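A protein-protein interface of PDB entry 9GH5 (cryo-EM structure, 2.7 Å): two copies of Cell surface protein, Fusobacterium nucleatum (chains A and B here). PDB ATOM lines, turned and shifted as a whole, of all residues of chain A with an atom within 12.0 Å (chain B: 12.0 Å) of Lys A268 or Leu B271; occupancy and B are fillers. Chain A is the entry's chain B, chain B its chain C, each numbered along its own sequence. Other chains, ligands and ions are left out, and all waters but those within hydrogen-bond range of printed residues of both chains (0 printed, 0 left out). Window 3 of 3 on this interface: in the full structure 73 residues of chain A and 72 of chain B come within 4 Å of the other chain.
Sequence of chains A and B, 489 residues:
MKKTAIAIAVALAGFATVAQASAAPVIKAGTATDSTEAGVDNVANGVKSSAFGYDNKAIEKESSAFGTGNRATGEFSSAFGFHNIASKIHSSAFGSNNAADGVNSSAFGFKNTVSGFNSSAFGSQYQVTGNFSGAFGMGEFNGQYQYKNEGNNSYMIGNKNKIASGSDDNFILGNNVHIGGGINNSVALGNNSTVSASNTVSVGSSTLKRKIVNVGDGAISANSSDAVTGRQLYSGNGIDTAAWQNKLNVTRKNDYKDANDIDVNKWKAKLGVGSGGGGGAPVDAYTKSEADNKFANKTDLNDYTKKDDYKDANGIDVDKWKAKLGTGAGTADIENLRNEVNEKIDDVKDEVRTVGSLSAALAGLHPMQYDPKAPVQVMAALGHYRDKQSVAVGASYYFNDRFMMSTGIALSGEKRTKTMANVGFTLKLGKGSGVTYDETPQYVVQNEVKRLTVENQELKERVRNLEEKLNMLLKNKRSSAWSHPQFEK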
ATOM      1  N   ASP A 255      -4.627   5.667 -26.982  1.00  0.00           N
ATOM      2  CA  ASP A 255      -3.866   4.649 -26.267  1.00  0.00           C
ATOM      3  C   ASP A 255      -2.565   5.213 -25.713  1.00  0.00           C
ATOM      4  O   ASP A 255      -2.159   4.866 -24.599  1.00  0.00           O
ATOM      5  CB  ASP A 255      -3.584   3.458 -27.182  1.00  0.00           C
ATOM      6  CG  ASP A 255      -4.834   2.671 -27.512  1.00  0.00           C
ATOM      7  OD1 ASP A 255      -5.920   3.046 -27.022  1.00  0.00           O
ATOM      8  OD2 ASP A 255      -4.731   1.679 -28.262  1.00  0.00           O
ATOM      9  N   TYR A 256      -1.898   6.082 -26.477  1.00  0.00           N
ATOM     10  CA  TYR A 256      -0.685   6.734 -26.004  1.00  0.00           C
ATOM     11  C   TYR A 256      -0.966   7.626 -24.800  1.00  0.00           C
ATOM     12  O   TYR A 256      -0.035   7.996 -24.080  1.00  0.00           O
ATOM     13  CB  TYR A 256      -0.074   7.563 -27.139  1.00  0.00           C
ATOM     14  CG  TYR A 256       1.110   8.423 -26.749  1.00  0.00           C
ATOM     15  CD1 TYR A 256       2.140   7.908 -25.971  1.00  0.00           C
ATOM     16  CD2 TYR A 256       1.173   9.759 -27.116  1.00  0.00           C
ATOM     17  CE1 TYR A 256       3.217   8.686 -25.608  1.00  0.00           C
ATOM     18  CE2 TYR A 256       2.247  10.547 -26.753  1.00  0.00           C
ATOM     19  CZ  TYR A 256       3.265  10.006 -25.998  1.00  0.00           C
ATOM     20  OH  TYR A 256       4.335  10.789 -25.630  1.00  0.00           O
ATOM     21  N   LYS A 257      -2.228   7.988 -24.579  1.00  0.00           N
ATOM     22  CA  LYS A 257      -2.633   8.755 -23.414  1.00  0.00           C
ATOM     23  C   LYS A 257      -3.140   7.884 -22.274  1.00  0.00           C
ATOM     24  O   LYS A 257      -2.992   8.267 -21.109  1.00  0.00           O
ATOM     25  CB  LYS A 257      -3.728   9.758 -23.809  1.00  0.00           C
ATOM     26  CG  LYS A 257      -4.174  10.704 -22.703  1.00  0.00           C
ATOM     27  CD  LYS A 257      -2.997  11.389 -22.033  1.00  0.00           C
ATOM     28  CE  LYS A 257      -2.224  12.243 -23.019  1.00  0.00           C
ATOM     29  NZ  LYS A 257      -1.720  13.497 -22.394  1.00  0.00           N
ATOM     30  N   ASP A 258      -3.711   6.718 -22.579  1.00  0.00           N
ATOM     31  CA  ASP A 258      -4.337   5.872 -21.570  1.00  0.00           C
ATOM     32  C   ASP A 258      -3.548   4.600 -21.277  1.00  0.00           C
ATOM     33  O   ASP A 258      -4.045   3.734 -20.547  1.00  0.00           O
ATOM     34  CB  ASP A 258      -5.767   5.522 -21.990  1.00  0.00           C
ATOM     35  CG  ASP A 258      -6.753   6.626 -21.667  1.00  0.00           C
ATOM     36  OD1 ASP A 258      -6.430   7.485 -20.819  1.00  0.00           O
ATOM     37  OD2 ASP A 258      -7.851   6.638 -22.262  1.00  0.00           O
ATOM     38  N   ALA A 259      -2.337   4.467 -21.822  1.00  0.00           N
ATOM     39  CA  ALA A 259      -1.442   3.342 -21.533  1.00  0.00           C
ATOM     40  C   ALA A 259      -2.046   2.000 -21.933  1.00  0.00           C
ATOM     41  O   ALA A 259      -1.745   0.968 -21.329  1.00  0.00           O
ATOM     42  CB  ALA A 259      -1.031   3.321 -20.056  1.00  0.00           C
ATOM     43  N   ASN A 260      -2.899   1.998 -22.953  1.00  0.00           N
ATOM     44  CA  ASN A 260      -3.461   0.750 -23.445  1.00  0.00           C
ATOM     45  C   ASN A 260      -2.435  -0.021 -24.266  1.00  0.00           C
ATOM     46  O   ASN A 260      -1.642   0.565 -25.009  1.00  0.00           O
ATOM     47  CB  ASN A 260      -4.705   1.021 -24.290  1.00  0.00           C
ATOM     48  CG  ASN A 260      -5.578   2.110 -23.708  1.00  0.00           C
ATOM     49  OD1 ASN A 260      -5.493   2.418 -22.521  1.00  0.00           O
ATOM     50  ND2 ASN A 260      -6.423   2.703 -24.544  1.00  0.00           N
ATOM     51  N   ASP A 261      -2.461  -1.347 -24.124  1.00  0.00           N
ATOM     52  CA  ASP A 261      -1.714  -2.274 -24.974  1.00  0.00           C
ATOM     53  C   ASP A 261      -0.210  -1.968 -24.891  1.00  0.00           C
ATOM     54  O   ASP A 261       0.420  -1.446 -25.813  1.00  0.00           O
ATOM     55  CB  ASP A 261      -2.282  -2.225 -26.406  1.00  0.00           C
ATOM     56  CG  ASP A 261      -1.316  -2.731 -27.479  1.00  0.00           C
ATOM     57  OD1 ASP A 261      -0.420  -3.547 -27.178  1.00  0.00           O
ATOM     58  OD2 ASP A 261      -1.458  -2.298 -28.641  1.00  0.00           O
ATOM     59  N   ILE A 262       0.331  -2.220 -23.699  1.00  0.00           N
ATOM     60  CA  ILE A 262       1.772  -2.214 -23.481  1.00  0.00           C
ATOM     61  C   ILE A 262       2.139  -3.430 -22.644  1.00  0.00           C
ATOM     62  O   ILE A 262       1.301  -4.002 -21.940  1.00  0.00           O
ATOM     63  CB  ILE A 262       2.280  -0.928 -22.788  1.00  0.00           C
ATOM     64  CG1 ILE A 262       1.944  -0.944 -21.297  1.00  0.00           C
ATOM     65  CG2 ILE A 262       1.707   0.311 -23.442  1.00  0.00           C
ATOM     66  CD1 ILE A 262       2.140   0.393 -20.623  1.00  0.00           C
ATOM     67  N   ASP A 263       3.403  -3.832 -22.735  1.00  0.00           N
ATOM     68  CA  ASP A 263       3.918  -4.863 -21.849  1.00  0.00           C
ATOM     69  C   ASP A 263       4.294  -4.258 -20.501  1.00  0.00           C
ATOM     70  O   ASP A 263       4.804  -3.140 -20.418  1.00  0.00           O
ATOM     71  CB  ASP A 263       5.135  -5.548 -22.470  1.00  0.00           C
ATOM     72  CG  ASP A 263       4.792  -6.315 -23.731  1.00  0.00           C
ATOM     73  OD1 ASP A 263       3.605  -6.651 -23.919  1.00  0.00           O
ATOM     74  OD2 ASP A 263       5.712  -6.585 -24.532  1.00  0.00           O
ATOM     75  N   VAL A 264       4.031  -5.009 -19.434  1.00  0.00           N
ATOM     76  CA  VAL A 264       4.412  -4.583 -18.099  1.00  0.00           C
ATOM     77  C   VAL A 264       5.684  -5.268 -17.611  1.00  0.00           C
ATOM     78  O   VAL A 264       6.422  -4.678 -16.814  1.00  0.00           O
ATOM     79  CB  VAL A 264       3.257  -4.791 -17.095  1.00  0.00           C
ATOM     80  CG1 VAL A 264       1.961  -4.232 -17.659  1.00  0.00           C
ATOM     81  CG2 VAL A 264       3.095  -6.263 -16.747  1.00  0.00           C
ATOM     82  N   ASN A 265       5.971  -6.487 -18.068  1.00  0.00           N
ATOM     83  CA  ASN A 265       7.216  -7.154 -17.719  1.00  0.00           C
ATOM     84  C   ASN A 265       8.398  -6.645 -18.530  1.00  0.00           C
ATOM     85  O   ASN A 265       9.543  -6.977 -18.205  1.00  0.00           O
ATOM     86  CB  ASN A 265       7.072  -8.666 -17.910  1.00  0.00           C
ATOM     87  CG  ASN A 265       6.497  -9.352 -16.688  1.00  0.00           C
ATOM     88  OD1 ASN A 265       6.536  -8.812 -15.584  1.00  0.00           O
ATOM     89  ND2 ASN A 265       5.955 -10.548 -16.883  1.00  0.00           N
ATOM     90  N   LYS A 266       8.147  -5.852 -19.570  1.00  0.00           N
ATOM     91  CA  LYS A 266       9.189  -5.304 -20.427  1.00  0.00           C
ATOM     92  C   LYS A 266       9.413  -3.817 -20.194  1.00  0.00           C
ATOM     93  O   LYS A 266      10.563  -3.371 -20.125  1.00  0.00           O
ATOM     94  CB  LYS A 266       8.833  -5.575 -21.899  1.00  0.00           C
ATOM     95  CG  LYS A 266       9.909  -5.222 -22.928  1.00  0.00           C
ATOM     96  CD  LYS A 266       9.820  -3.764 -23.359  1.00  0.00           C
ATOM     97  CE  LYS A 266       8.374  -3.291 -23.346  1.00  0.00           C
ATOM     98  NZ  LYS A 266       8.240  -1.879 -23.770  1.00  0.00           N
ATOM     99  N   TRP A 267       8.339  -3.030 -20.087  1.00  0.00           N
ATOM    100  CA  TRP A 267       8.498  -1.607 -19.797  1.00  0.00           C
ATOM    101  C   TRP A 267       9.161  -1.401 -18.443  1.00  0.00           C
ATOM    102  O   TRP A 267       9.988  -0.497 -18.278  1.00  0.00           O
ATOM    103  CB  TRP A 267       7.144  -0.895 -19.841  1.00  0.00           C
ATOM    104  CG  TRP A 267       6.735  -0.404 -21.203  1.00  0.00           C
ATOM    105  CD1 TRP A 267       5.937  -1.049 -22.102  1.00  0.00           C
ATOM    106  CD2 TRP A 267       7.102   0.839 -21.815  1.00  0.00           C
ATOM    107  NE1 TRP A 267       5.787  -0.288 -23.235  1.00  0.00           N
ATOM    108  CE2 TRP A 267       6.492   0.876 -23.084  1.00  0.00           C
ATOM    109  CE3 TRP A 267       7.888   1.922 -21.413  1.00  0.00           C
ATOM    110  CZ2 TRP A 267       6.643   1.953 -23.952  1.00  0.00           C
ATOM    111  CZ3 TRP A 267       8.037   2.990 -22.277  1.00  0.00           C
ATOM    112  CH2 TRP A 267       7.417   2.998 -23.532  1.00  0.00           C
ATOM    113  N   LYS A 268       8.809  -2.233 -17.460  1.00  0.00           N
ATOM    114  CA  LYS A 268       9.435  -2.154 -16.146  1.00  0.00           C
ATOM    115  C   LYS A 268      10.930  -2.435 -16.199  1.00  0.00           C
ATOM    116  O   LYS A 268      11.656  -2.028 -15.286  1.00  0.00           O
ATOM    117  CB  LYS A 268       8.764  -3.136 -15.184  1.00  0.00           C
ATOM    118  CG  LYS A 268       7.862  -2.488 -14.147  1.00  0.00           C
ATOM    119  CD  LYS A 268       6.450  -2.315 -14.676  1.00  0.00           C
ATOM    120  CE  LYS A 268       5.508  -1.831 -13.590  1.00  0.00           C
ATOM    121  NZ  LYS A 268       4.082  -1.949 -14.001  1.00  0.00           N
ATOM    122  N   ALA A 269      11.406  -3.125 -17.235  1.00  0.00           N
ATOM    123  CA  ALA A 269      12.828  -3.435 -17.332  1.00  0.00           C
ATOM    124  C   ALA A 269      13.645  -2.192 -17.668  1.00  0.00           C
ATOM    125  O   ALA A 269      14.535  -1.796 -16.909  1.00  0.00           O
ATOM    126  CB  ALA A 269      13.057  -4.530 -18.377  1.00  0.00           C
ATOM    127  N   LYS A 270      13.354  -1.565 -18.810  1.00  0.00           N
ATOM    128  CA  LYS A 270      14.124  -0.398 -19.227  1.00  0.00           C
ATOM    129  C   LYS A 270      13.841   0.806 -18.337  1.00  0.00           C
ATOM    130  O   LYS A 270      14.735   1.625 -18.091  1.00  0.00           O
ATOM    131  CB  LYS A 270      13.826  -0.069 -20.690  1.00  0.00           C
ATOM    132  CG  LYS A 270      14.522  -0.991 -21.680  1.00  0.00           C
ATOM    133  CD  LYS A 270      14.916  -0.263 -22.957  1.00  0.00           C
ATOM    134  CE  LYS A 270      13.909   0.812 -23.331  1.00  0.00           C
ATOM    135  NZ  LYS A 270      13.845   1.016 -24.803  1.00  0.00           N
ATOM    136  N   LEU A 271      12.611   0.934 -17.847  1.00  0.00           N
ATOM    137  CA  LEU A 271      12.212   2.077 -17.039  1.00  0.00           C
ATOM    138  C   LEU A 271      12.291   1.807 -15.540  1.00  0.00           C
ATOM    139  O   LEU A 271      11.871   2.656 -14.749  1.00  0.00           O
ATOM    140  CB  LEU A 271      10.794   2.526 -17.409  1.00  0.00           C
ATOM    141  CG  LEU A 271      10.603   3.402 -18.654  1.00  0.00           C
ATOM    142  CD1 LEU A 271      11.307   4.739 -18.472  1.00  0.00           C
ATOM    143  CD2 LEU A 271      11.065   2.717 -19.936  1.00  0.00           C
ATOM    144  N   GLY A 272      12.814   0.656 -15.135  1.00  0.00           N
ATOM    145  CA  GLY A 272      12.957   0.346 -13.724  1.00  0.00           C
ATOM    146  C   GLY A 272      11.635   0.084 -13.031  1.00  0.00           C
ATOM    147  O   GLY A 272      11.505   0.284 -11.823  1.00  0.00           O
ATOM    148  N   TYR B 256       6.779  10.684 -28.793  1.00  0.00           N
ATOM    149  CA  TYR B 256       6.898   9.386 -28.135  1.00  0.00           C
ATOM    150  C   TYR B 256       8.278   9.218 -27.515  1.00  0.00           C
ATOM    151  O   TYR B 256       8.403   8.779 -26.366  1.00  0.00           O
ATOM    152  CB  TYR B 256       6.621   8.275 -29.147  1.00  0.00           C
ATOM    153  CG  TYR B 256       7.190   6.917 -28.796  1.00  0.00           C
ATOM    154  CD1 TYR B 256       6.918   6.318 -27.571  1.00  0.00           C
ATOM    155  CD2 TYR B 256       8.014   6.241 -29.684  1.00  0.00           C
ATOM    156  CE1 TYR B 256       7.433   5.076 -27.254  1.00  0.00           C
ATOM    157  CE2 TYR B 256       8.534   5.002 -29.374  1.00  0.00           C
ATOM    158  CZ  TYR B 256       8.243   4.425 -28.159  1.00  0.00           C
ATOM    159  OH  TYR B 256       8.761   3.189 -27.850  1.00  0.00           O
ATOM    160  N   ALA B 259       8.477  11.845 -24.581  1.00  0.00           N
ATOM    161  CA  ALA B 259       7.471  11.716 -23.526  1.00  0.00           C
ATOM    162  C   ALA B 259       6.492  12.885 -23.496  1.00  0.00           C
ATOM    163  O   ALA B 259       5.884  13.160 -22.458  1.00  0.00           O
ATOM    164  CB  ALA B 259       8.123  11.547 -22.148  1.00  0.00           C
ATOM    165  N   ILE B 262       1.454  13.132 -22.261  1.00  0.00           N
ATOM    166  CA  ILE B 262       1.119  11.895 -21.561  1.00  0.00           C
ATOM    167  C   ILE B 262       0.494  12.240 -20.218  1.00  0.00           C
ATOM    168  O   ILE B 262       0.804  13.278 -19.624  1.00  0.00           O
ATOM    169  CB  ILE B 262       2.351  10.989 -21.345  1.00  0.00           C
ATOM    170  CG1 ILE B 262       3.446  11.736 -20.583  1.00  0.00           C
ATOM    171  CG2 ILE B 262       2.883  10.475 -22.663  1.00  0.00           C
ATOM    172  CD1 ILE B 262       4.723  10.940 -20.425  1.00  0.00           C
ATOM    173  N   ASP B 263      -0.394  11.370 -19.744  1.00  0.00           N
ATOM    174  CA  ASP B 263      -0.823  11.439 -18.356  1.00  0.00           C
ATOM    175  C   ASP B 263       0.291  10.943 -17.443  1.00  0.00           C
ATOM    176  O   ASP B 263       1.085  10.072 -17.808  1.00  0.00           O
ATOM    177  CB  ASP B 263      -2.086  10.607 -18.136  1.00  0.00           C
ATOM    178  CG  ASP B 263      -3.328  11.272 -18.691  1.00  0.00           C
ATOM    179  OD1 ASP B 263      -3.311  12.507 -18.874  1.00  0.00           O
ATOM    180  OD2 ASP B 263      -4.321  10.560 -18.948  1.00  0.00           O
ATOM    181  N   VAL B 264       0.350  11.510 -16.241  1.00  0.00           N
ATOM    182  CA  VAL B 264       1.342  11.131 -15.250  1.00  0.00           C
ATOM    183  C   VAL B 264       0.712  10.400 -14.069  1.00  0.00           C
ATOM    184  O   VAL B 264       1.289   9.441 -13.555  1.00  0.00           O
ATOM    185  CB  VAL B 264       2.156  12.358 -14.778  1.00  0.00           C
ATOM    186  CG1 VAL B 264       2.853  13.008 -15.961  1.00  0.00           C
ATOM    187  CG2 VAL B 264       1.265  13.373 -14.077  1.00  0.00           C
ATOM    188  N   ASN B 265      -0.475  10.826 -13.633  1.00  0.00           N
ATOM    189  CA  ASN B 265      -1.160  10.148 -12.541  1.00  0.00           C
ATOM    190  C   ASN B 265      -1.605   8.741 -12.910  1.00  0.00           C
ATOM    191  O   ASN B 265      -1.847   7.929 -12.009  1.00  0.00           O
ATOM    192  CB  ASN B 265      -2.368  10.970 -12.091  1.00  0.00           C
ATOM    193  CG  ASN B 265      -3.522  10.900 -13.076  1.00  0.00           C
ATOM    194  OD1 ASN B 265      -3.322  10.709 -14.275  1.00  0.00           O
ATOM    195  ND2 ASN B 265      -4.740  11.050 -12.569  1.00  0.00           N
ATOM    196  N   LYS B 266      -1.716   8.435 -14.198  1.00  0.00           N
ATOM    197  CA  LYS B 266      -2.190   7.143 -14.676  1.00  0.00           C
ATOM    198  C   LYS B 266      -1.081   6.249 -15.205  1.00  0.00           C
ATOM    199  O   LYS B 266      -1.142   5.031 -15.024  1.00  0.00           O
ATOM    200  CB  LYS B 266      -3.245   7.352 -15.764  1.00  0.00           C
ATOM    201  CG  LYS B 266      -4.068   6.121 -16.095  1.00  0.00           C
ATOM    202  CD  LYS B 266      -4.886   6.348 -17.354  1.00  0.00           C
ATOM    203  CE  LYS B 266      -4.151   7.260 -18.324  1.00  0.00           C
ATOM    204  NZ  LYS B 266      -2.893   6.643 -18.834  1.00  0.00           N
ATOM    205  N   TRP B 267      -0.069   6.817 -15.866  1.00  0.00           N
ATOM    206  CA  TRP B 267       1.117   6.034 -16.200  1.00  0.00           C
ATOM    207  C   TRP B 267       1.809   5.525 -14.944  1.00  0.00           C
ATOM    208  O   TRP B 267       2.211   4.357 -14.879  1.00  0.00           O
ATOM    209  CB  TRP B 267       2.084   6.862 -17.043  1.00  0.00           C
ATOM    210  CG  TRP B 267       2.408   6.248 -18.368  1.00  0.00           C
ATOM    211  CD1 TRP B 267       3.531   5.543 -18.684  1.00  0.00           C
ATOM    212  CD2 TRP B 267       1.610   6.284 -19.555  1.00  0.00           C
ATOM    213  NE1 TRP B 267       3.483   5.134 -19.993  1.00  0.00           N
ATOM    214  CE2 TRP B 267       2.314   5.577 -20.551  1.00  0.00           C
ATOM    215  CE3 TRP B 267       0.371   6.843 -19.874  1.00  0.00           C
ATOM    216  CZ2 TRP B 267       1.821   5.416 -21.839  1.00  0.00           C
ATOM    217  CZ3 TRP B 267      -0.115   6.682 -21.154  1.00  0.00           C
ATOM    218  CH2 TRP B 267       0.608   5.973 -22.120  1.00  0.00           C
ATOM    219  N   LYS B 268       1.956   6.385 -13.934  1.00  0.00           N
ATOM    220  CA  LYS B 268       2.568   5.959 -12.681  1.00  0.00           C
ATOM    221  C   LYS B 268       1.750   4.886 -11.977  1.00  0.00           C
ATOM    222  O   LYS B 268       2.287   4.177 -11.121  1.00  0.00           O
ATOM    223  CB  LYS B 268       2.760   7.158 -11.751  1.00  0.00           C
ATOM    224  CG  LYS B 268       3.806   8.155 -12.221  1.00  0.00           C
ATOM    225  CD  LYS B 268       5.134   7.946 -11.515  1.00  0.00           C
ATOM    226  CE  LYS B 268       5.713   9.269 -11.044  1.00  0.00           C
ATOM    227  NZ  LYS B 268       6.057  10.168 -12.179  1.00  0.00           N
ATOM    228  N   ALA B 269       0.464   4.757 -12.309  1.00  0.00           N
ATOM    229  CA  ALA B 269      -0.358   3.713 -11.709  1.00  0.00           C
ATOM    230  C   ALA B 269       0.015   2.337 -12.251  1.00  0.00           C
ATOM    231  O   ALA B 269       0.405   1.442 -11.494  1.00  0.00           O
ATOM    232  CB  ALA B 269      -1.840   4.008 -11.953  1.00  0.00           C
ATOM    233  N   LYS B 270      -0.102   2.153 -13.568  1.00  0.00           N
ATOM    234  CA  LYS B 270       0.195   0.852 -14.159  1.00  0.00           C
ATOM    235  C   LYS B 270       1.692   0.562 -14.142  1.00  0.00           C
ATOM    236  O   LYS B 270       2.105  -0.577 -13.892  1.00  0.00           O
ATOM    237  CB  LYS B 270      -0.362   0.788 -15.583  1.00  0.00           C
ATOM    238  CG  LYS B 270       0.455  -0.049 -16.549  1.00  0.00           C
ATOM    239  CD  LYS B 270      -0.160  -0.057 -17.939  1.00  0.00           C
ATOM    240  CE  LYS B 270      -1.668  -0.241 -17.889  1.00  0.00           C
ATOM    241  NZ  LYS B 270      -2.281  -0.113 -19.241  1.00  0.00           N
ATOM    242  N   LEU B 271       2.522   1.577 -14.392  1.00  0.00           N
ATOM    243  CA  LEU B 271       3.968   1.391 -14.395  1.00  0.00           C
ATOM    244  C   LEU B 271       4.590   1.489 -13.008  1.00  0.00           C
ATOM    245  O   LEU B 271       5.807   1.313 -12.884  1.00  0.00           O
ATOM    246  CB  LEU B 271       4.642   2.412 -15.319  1.00  0.00           C
ATOM    247  CG  LEU B 271       4.822   2.090 -16.806  1.00  0.00           C
ATOM    248  CD1 LEU B 271       6.093   1.283 -17.015  1.00  0.00           C
ATOM    249  CD2 LEU B 271       3.625   1.359 -17.389  1.00  0.00           C
ATOM    250  N   GLY B 272       3.802   1.763 -11.976  1.00  0.00           N
ATOM    251  CA  GLY B 272       4.335   1.871 -10.629  1.00  0.00           C
ATOM    252  C   GLY B 272       5.139   3.137 -10.414  1.00  0.00           C
ATOM    253  O   GLY B 272       5.810   3.295  -9.394  1.00  0.00           O
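The side-chain amino group of Lys A268 sits at hydrogen-bond distance from the backbone carbonyl oxygen of Lys B270.
The backbone carbonyl oxygen (O) of Ala A259 lies within hydrogen-bond range of the side-chain amino group (NZ) of Lys B270 (2.4 Å).
The side-chain amino group of Lys A257 lies within salt-bridge range of the side-chain carboxylate of Asp B263, 3.99 Å away.
O of Lys A257 lies within hydrogen-bond range of NZ of Lys B266 (2.8 Å).
The backbone NH (N) of Ile B262 lies close to the side-chain amino group (NZ) of Lys A257, 3.2 Å away.
The side-chain amide oxygen of Asn A260 lies close to the backbone carbonyl oxygen of Asp A258 (2.8 Å).
OD1 of Asp A255 sits at hydrogen-bond distance from ND2 of Asn A260, 2.6 Å away.
Among the printed residues, merely in contact across the chains: Asp A255 with Trp B267 (3.9 Å), Tyr A256 with Tyr B256 (3.8 Å), Tyr A256 with Ala B259 (3.7 Å), Tyr A256 with Ile B262 (3.3 Å), Tyr A256 with Trp B267 (2.9 Å), Lys A257 with Trp B267 (3.3 Å), Asp A258 with Lys B266 (3.2 Å), Asp A258 with Trp B267 (3.9 Å), Ala A259 with Lys B266 (3.7 Å), Ala A259 with Trp B267 (3.2 Å), Ile A262 with Lys B270 (3.6 Å), Ile A262 with Leu B271 (3.7 Å), Trp A267 with Leu B271 (3.7 Å) and Lys A268 with Leu B271 (3.2 Å).
Lys A268 touches just these residues of chain B: Lys B270 (2.4 Å) and Leu B271 (3.2 Å).
No residue of chain B comes within 4 Å of Val A264.
Lys A266 touches none of the printed residues of chain B.
No residue of chain B comes within 4 Å of Ala A269.
No residue of chain B comes within 4 Å of Leu A271.
Of chain A, only Asp A255, Tyr A256, Lys A257, Asp A258 and Ala A259 come within 4 Å of Trp B267.
No residue of chain A comes within 4 Å of Ala B269.
Of chain A, only Ala A259, Ile A262 and Lys A268 come within 4 Å of Lys B270.
No residue of chain A comes within 4 Å of Gly B272.
Printed residues of chain A within 4 Å of Tyr B256: Tyr A256 (3.8 Å).
Of the printed residues of chain B, Ala A259 touches Lys B266 (3.7 Å), Trp B267 (3.2 Å) and Lys B270 (2.4 Å).
Printed residues of chain A within 4 Å of Lys B266: Lys A257 (2.8 Å), Asp A258 (3.2 Å) and Ala A259 (3.7 Å).
Printed residues of chain A within 4 Å of Asp B263: Lys A257 (3.4 Å).
Printed residues of chain A within 4 Å of Ile B262: Tyr A256 (3.3 Å) and Lys A257 (3.2 Å).
Asp A263 touches none of the printed residues of chain B.
Asn A265 touches none of the printed residues of chain B.
The nearest residue of chain B that does not touch Lys A268 is Gly B272 (4.2 Å).
The nearest printed residue of chain B that does not touch Ile A262 is Trp B267 (5.0 Å).
Of the 18 printed residues of chain A, 8 touch a printed residue of chain B.
Printed residues of chain A that touch a printed residue of chain B: Asp A255, Tyr A256, Lys A257, Asp A258, Ala A259, Ile A262, Trp A267 and Lys A268.
Of the 13 printed residues of chain B, 8 touch a printed residue of chain A.
Printed residues of chain B that touch a printed residue of chain A: Tyr B256, Ala B259, Ile B262, Asp B263, Lys B266, Trp B267, Lys B270 and Leu B271.
Tyr A256 touches Ala B259, but with the chains exchanged Ala A259 does not touch Tyr B256 (10.7 Å).
Tyr A256 touches Ile B262, but with the chains exchanged Ile A262 does not touch Tyr B256 (8.4 Å).
Lys A268 touches Lys B270, but with the chains exchanged Lys A270 does not touch Lys B268 (13.2 Å).
Lys A268 touches Leu B271, but with the chains exchanged Leu A271 does not touch Lys B268 (9.2 Å).
Positions printed for both chains: 256, 259, 262, 263, 264, 265, 266, 267, 268, 269, 270, 271 and 272.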
